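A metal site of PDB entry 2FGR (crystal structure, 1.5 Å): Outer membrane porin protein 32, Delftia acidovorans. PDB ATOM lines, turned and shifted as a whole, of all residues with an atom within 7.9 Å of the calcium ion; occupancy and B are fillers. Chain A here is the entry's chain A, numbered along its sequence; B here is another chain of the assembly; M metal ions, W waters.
O of Asn 136 of chain B lies within hydrogen-bond range of N of Phe 156 of chain B (3.1 Å).
Of the 20 residues printed, 5 come within 4 Å of the calcium ion. The nearest printed residue that does not touch the calcium ion is Val 310 (4.5 Å).
The calcium ion is bound by the backbone carbonyl oxygen (O) of Gly 309 (2.3 Å), the side-chain carboxylate (OD2) of Asp 64 (2.3 Å), the side-chain amide oxygen (OD1) of Asn 136 of chain B (2.3 Å), the backbone carbonyl oxygen (O) of Leu 29 (2.4 Å), water W1 (2.4 Å), the side-chain carboxylate (OE2) of Glu 158 of chain B (2.5 Å) and the side-chain carboxylate (OE1) of Glu 158 of chain B (2.5 Å). The calcium ion has seven donor atoms within binding distance.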
ATOM      1  N   ASN A  13     -12.828  31.123 -16.297  1.00  0.00           N
ATOM      2  CA  ASN A  13     -13.695  31.200 -15.116  1.00  0.00           C
ATOM      3  C   ASN A  13     -12.870  31.485 -13.881  1.00  0.00           C
ATOM      4  O   ASN A  13     -11.651  31.344 -13.876  1.00  0.00           O
ATOM      5  CB  ASN A  13     -14.526  29.943 -14.908  1.00  0.00           C
ATOM      6  CG  ASN A  13     -13.696  28.651 -14.855  1.00  0.00           C
ATOM      7  OD1 ASN A  13     -12.774  28.522 -14.046  1.00  0.00           O
ATOM      8  ND2 ASN A  13     -14.017  27.694 -15.746  1.00  0.00           N
ATOM      9  N   TYR A  27      -8.796  28.065  -4.776  1.00  0.00           N
ATOM     10  CA  TYR A  27      -9.537  28.906  -5.677  1.00  0.00           C
ATOM     11  C   TYR A  27      -8.578  29.554  -6.660  1.00  0.00           C
ATOM     12  O   TYR A  27      -7.371  29.614  -6.426  1.00  0.00           O
ATOM     13  CB  TYR A  27     -10.369  29.908  -4.926  1.00  0.00           C
ATOM     14  CG  TYR A  27      -9.542  30.863  -4.121  1.00  0.00           C
ATOM     15  CD1 TYR A  27      -9.145  32.063  -4.651  1.00  0.00           C
ATOM     16  CD2 TYR A  27      -9.144  30.534  -2.824  1.00  0.00           C
ATOM     17  CE1 TYR A  27      -8.383  32.963  -3.939  1.00  0.00           C
ATOM     18  CE2 TYR A  27      -8.328  31.436  -2.082  1.00  0.00           C
ATOM     19  CZ  TYR A  27      -7.960  32.645  -2.656  1.00  0.00           C
ATOM     20  OH  TYR A  27      -7.177  33.570  -1.975  1.00  0.00           O
ATOM     21  N   GLY A  28      -9.120  29.968  -7.792  1.00  0.00           N
ATOM     22  CA  GLY A  28      -8.256  30.509  -8.788  1.00  0.00           C
ATOM     23  C   GLY A  28      -8.974  30.777 -10.093  1.00  0.00           C
ATOM     24  O   GLY A  28     -10.171  30.881 -10.131  1.00  0.00           O
ATOM     25  N   LEU A  29      -8.193  30.991 -11.127  1.00  0.00           N
ATOM     26  CA  LEU A  29      -8.699  31.232 -12.490  1.00  0.00           C
ATOM     27  C   LEU A  29      -8.524  29.921 -13.215  1.00  0.00           C
ATOM     28  O   LEU A  29      -7.416  29.408 -13.337  1.00  0.00           O
ATOM     29  CB  LEU A  29      -7.880  32.326 -13.186  1.00  0.00           C
ATOM     30  CG  LEU A  29      -8.636  32.928 -14.399  1.00  0.00           C
ATOM     31  CD1 LEU A  29      -9.680  33.951 -13.969  1.00  0.00           C
ATOM     32  CD2 LEU A  29      -7.658  33.577 -15.367  1.00  0.00           C
ATOM     33  N   GLY A  30      -9.619  29.385 -13.701  1.00  0.00           N
ATOM     34  CA  GLY A  30      -9.589  28.147 -14.472  1.00  0.00           C
ATOM     35  C   GLY A  30     -10.190  28.343 -15.845  1.00  0.00           C
ATOM     36  O   GLY A  30     -10.406  29.457 -16.309  1.00  0.00           O
ATOM     37  N   THR A  31     -10.485  27.230 -16.506  1.00  0.00           N
ATOM     38  CA  THR A  31     -10.934  27.224 -17.878  1.00  0.00           C
ATOM     39  C   THR A  31     -12.013  26.226 -18.131  1.00  0.00           C
ATOM     40  O   THR A  31     -12.215  25.253 -17.353  1.00  0.00           O
ATOM     41  CB  THR A  31      -9.787  26.961 -18.882  1.00  0.00           C
ATOM     42  OG1 THR A  31      -9.211  25.681 -18.655  1.00  0.00           O
ATOM     43  CG2 THR A  31      -8.659  27.950 -18.680  1.00  0.00           C
ATOM     44  N   GLY A  63      -6.553  29.366 -21.250  1.00  0.00           N
ATOM     45  CA  GLY A  63      -6.394  30.817 -21.183  1.00  0.00           C
ATOM     46  C   GLY A  63      -5.793  31.312 -19.894  1.00  0.00           C
ATOM     47  O   GLY A  63      -5.194  32.390 -19.846  1.00  0.00           O
ATOM     48  N   ASP A  64      -5.859  30.524 -18.831  1.00  0.00           N
ATOM     49  CA  ASP A  64      -5.257  30.956 -17.592  1.00  0.00           C
ATOM     50  C   ASP A  64      -3.723  30.952 -17.595  1.00  0.00           C
ATOM     51  O   ASP A  64      -3.109  31.661 -16.820  1.00  0.00           O
ATOM     52  CB  ASP A  64      -5.781  30.186 -16.366  1.00  0.00           C
ATOM     53  CG  ASP A  64      -5.545  28.691 -16.420  1.00  0.00           C
ATOM     54  OD1 ASP A  64      -5.370  28.088 -17.526  1.00  0.00           O
ATOM     55  OD2 ASP A  64      -5.510  28.011 -15.331  1.00  0.00           O
ATOM     56  N   ASP A  65      -3.092  30.151 -18.458  1.00  0.00           N
ATOM     57  CA  ASP A  65      -1.626  30.084 -18.526  1.00  0.00           C
ATOM     58  C   ASP A  65      -1.035  30.212 -19.907  1.00  0.00           C
ATOM     59  O   ASP A  65       0.163  30.003 -20.107  1.00  0.00           O
ATOM     60  CB  ASP A  65      -1.079  28.887 -17.774  1.00  0.00           C
ATOM     61  CG  ASP A  65      -1.307  27.571 -18.435  1.00  0.00           C
ATOM     62  OD1 ASP A  65      -1.629  27.462 -19.659  1.00  0.00           O
ATOM     63  OD2 ASP A  65      -1.093  26.522 -17.764  1.00  0.00           O
ATOM     64  N   ALA A 307     -12.345  21.024 -11.538  1.00  0.00           N
ATOM     65  CA  ALA A 307     -12.210  22.474 -11.761  1.00  0.00           C
ATOM     66  C   ALA A 307     -10.916  22.727 -12.545  1.00  0.00           C
ATOM     67  O   ALA A 307      -9.886  23.016 -11.958  1.00  0.00           O
ATOM     68  CB  ALA A 307     -12.202  23.242 -10.457  1.00  0.00           C
ATOM     69  N   LYS A 308     -11.007  22.574 -13.855  1.00  0.00           N
ATOM     70  CA  LYS A 308      -9.827  22.610 -14.689  1.00  0.00           C
ATOM     71  C   LYS A 308      -9.111  23.954 -14.524  1.00  0.00           C
ATOM     72  O   LYS A 308      -9.731  25.006 -14.592  1.00  0.00           O
ATOM     73  CB  LYS A 308     -10.169  22.402 -16.143  1.00  0.00           C
ATOM     74  CG  LYS A 308      -8.975  22.396 -17.052  1.00  0.00           C
ATOM     75  CD  LYS A 308      -9.379  22.036 -18.476  1.00  0.00           C
ATOM     76  CE  LYS A 308      -9.466  20.506 -18.653  1.00  0.00           C
ATOM     77  NZ  LYS A 308      -9.908  20.083 -19.997  1.00  0.00           N
ATOM     78  N   GLY A 309      -7.831  23.884 -14.285  1.00  0.00           N
ATOM     79  CA  GLY A 309      -7.001  25.055 -14.077  1.00  0.00           C
ATOM     80  C   GLY A 309      -6.968  25.572 -12.664  1.00  0.00           C
ATOM     81  O   GLY A 309      -6.259  26.533 -12.401  1.00  0.00           O
ATOM     82  N   VAL A 310      -7.707  24.955 -11.748  1.00  0.00           N
ATOM     83  CA  VAL A 310      -7.684  25.357 -10.336  1.00  0.00           C
ATOM     84  C   VAL A 310      -7.343  24.145  -9.503  1.00  0.00           C
ATOM     85  O   VAL A 310      -6.307  24.119  -8.872  1.00  0.00           O
ATOM     86  CB  VAL A 310      -8.993  26.002  -9.915  1.00  0.00           C
ATOM     87  CG1 VAL A 310      -8.958  26.319  -8.395  1.00  0.00           C
ATOM     88  CG2 VAL A 310      -9.169  27.331 -10.667  1.00  0.00           C
ATOM     89  N   TYR A 311      -8.226  23.132  -9.525  1.00  0.00           N
ATOM     90  CA  TYR A 311      -7.949  21.856  -8.839  1.00  0.00           C
ATOM     91  C   TYR A 311      -8.829  20.772  -9.400  1.00  0.00           C
ATOM     92  O   TYR A 311     -10.039  20.923  -9.467  1.00  0.00           O
ATOM     93  CB  TYR A 311      -8.142  21.991  -7.301  1.00  0.00           C
ATOM     94  CG  TYR A 311      -7.742  20.702  -6.580  1.00  0.00           C
ATOM     95  CD1 TYR A 311      -6.409  20.327  -6.471  1.00  0.00           C
ATOM     96  CD2 TYR A 311      -8.695  19.806  -6.122  1.00  0.00           C
ATOM     97  CE1 TYR A 311      -6.034  19.142  -5.865  1.00  0.00           C
ATOM     98  CE2 TYR A 311      -8.322  18.604  -5.511  1.00  0.00           C
ATOM     99  CZ  TYR A 311      -6.993  18.283  -5.389  1.00  0.00           C
ATOM    100  OH  TYR A 311      -6.593  17.084  -4.815  1.00  0.00           O
ATOM    101  N   ASN B 135       0.203  34.416 -14.898  1.00  0.00           N
ATOM    102  CA  ASN B 135      -0.869  33.439 -15.033  1.00  0.00           C
ATOM    103  C   ASN B 135      -2.065  33.801 -14.171  1.00  0.00           C
ATOM    104  O   ASN B 135      -1.927  34.484 -13.144  1.00  0.00           O
ATOM    105  CB  ASN B 135      -0.361  32.039 -14.605  1.00  0.00           C
ATOM    106  CG  ASN B 135       0.748  31.512 -15.469  1.00  0.00           C
ATOM    107  OD1 ASN B 135       1.697  30.813 -14.987  1.00  0.00           O
ATOM    108  ND2 ASN B 135       0.696  31.823 -16.688  1.00  0.00           N
ATOM    109  N   ASN B 136      -3.249  33.322 -14.503  1.00  0.00           N
ATOM    110  CA  ASN B 136      -4.366  33.379 -13.592  1.00  0.00           C
ATOM    111  C   ASN B 136      -4.790  34.817 -13.258  1.00  0.00           C
ATOM    112  O   ASN B 136      -5.255  35.091 -12.144  1.00  0.00           O
ATOM    113  CB  ASN B 136      -4.084  32.607 -12.285  1.00  0.00           C
ATOM    114  CG  ASN B 136      -3.541  31.201 -12.577  1.00  0.00           C
ATOM    115  OD1 ASN B 136      -4.108  30.497 -13.421  1.00  0.00           O
ATOM    116  ND2 ASN B 136      -2.436  30.818 -11.911  1.00  0.00           N
ATOM    117  N   LEU B 137      -4.670  35.694 -14.239  1.00  0.00           N
ATOM    118  CA  LEU B 137      -4.850  37.124 -14.070  1.00  0.00           C
ATOM    119  C   LEU B 137      -6.248  37.620 -14.399  1.00  0.00           C
ATOM    120  O   LEU B 137      -6.855  37.221 -15.421  1.00  0.00           O
ATOM    121  CB  LEU B 137      -3.827  37.841 -14.947  1.00  0.00           C
ATOM    122  CG  LEU B 137      -3.838  39.362 -14.953  1.00  0.00           C
ATOM    123  CD1 LEU B 137      -3.446  39.941 -13.597  1.00  0.00           C
ATOM    124  CD2 LEU B 137      -2.898  39.835 -16.023  1.00  0.00           C
ATOM    125  N   PHE B 156      -4.236  35.032  -9.193  1.00  0.00           N
ATOM    126  CA  PHE B 156      -4.359  33.974  -8.209  1.00  0.00           C
ATOM    127  C   PHE B 156      -3.117  33.114  -8.147  1.00  0.00           C
ATOM    128  O   PHE B 156      -2.626  32.643  -9.173  1.00  0.00           O
ATOM    129  CB  PHE B 156      -5.553  33.071  -8.504  1.00  0.00           C
ATOM    130  CG  PHE B 156      -6.872  33.757  -8.491  1.00  0.00           C
ATOM    131  CD1 PHE B 156      -7.409  34.259  -9.654  1.00  0.00           C
ATOM    132  CD2 PHE B 156      -7.602  33.911  -7.310  1.00  0.00           C
ATOM    133  CE1 PHE B 156      -8.661  34.891  -9.651  1.00  0.00           C
ATOM    134  CE2 PHE B 156      -8.826  34.532  -7.310  1.00  0.00           C
ATOM    135  CZ  PHE B 156      -9.362  35.026  -8.478  1.00  0.00           C
ATOM    136  N   ASP B 157      -2.638  32.835  -6.930  1.00  0.00           N
ATOM    137  CA  ASP B 157      -1.530  31.901  -6.727  1.00  0.00           C
ATOM    138  C   ASP B 157      -1.915  30.454  -6.821  1.00  0.00           C
ATOM    139  O   ASP B 157      -1.080  29.617  -7.167  1.00  0.00           O
ATOM    140  CB  ASP B 157      -0.896  32.132  -5.347  1.00  0.00           C
ATOM    141  CG  ASP B 157      -1.926  32.163  -4.255  1.00  0.00           C
ATOM    142  OD1 ASP B 157      -2.161  31.110  -3.602  1.00  0.00           O
ATOM    143  OD2 ASP B 157      -2.633  33.189  -4.034  1.00  0.00           O
ATOM    144  N   GLU B 158      -3.164  30.167  -6.493  1.00  0.00           N
ATOM    145  CA  GLU B 158      -3.705  28.797  -6.541  1.00  0.00           C
ATOM    146  C   GLU B 158      -2.884  27.820  -5.693  1.00  0.00           C
ATOM    147  O   GLU B 158      -2.744  26.633  -6.026  1.00  0.00           O
ATOM    148  CB  GLU B 158      -3.823  28.310  -7.994  1.00  0.00           C
ATOM    149  CG  GLU B 158      -4.610  29.279  -8.832  1.00  0.00           C
ATOM    150  CD  GLU B 158      -4.791  28.935 -10.304  1.00  0.00           C
ATOM    151  OE1 GLU B 158      -4.068  28.081 -10.889  1.00  0.00           O
ATOM    152  OE2 GLU B 158      -5.669  29.602 -10.907  1.00  0.00           O
HETATM  153 CA    CA M   1      -5.255  28.491 -13.059  1.00  0.00          CA
HETATM  154  O   HOH W   1      -3.247  27.238 -13.619  1.00  0.00           O
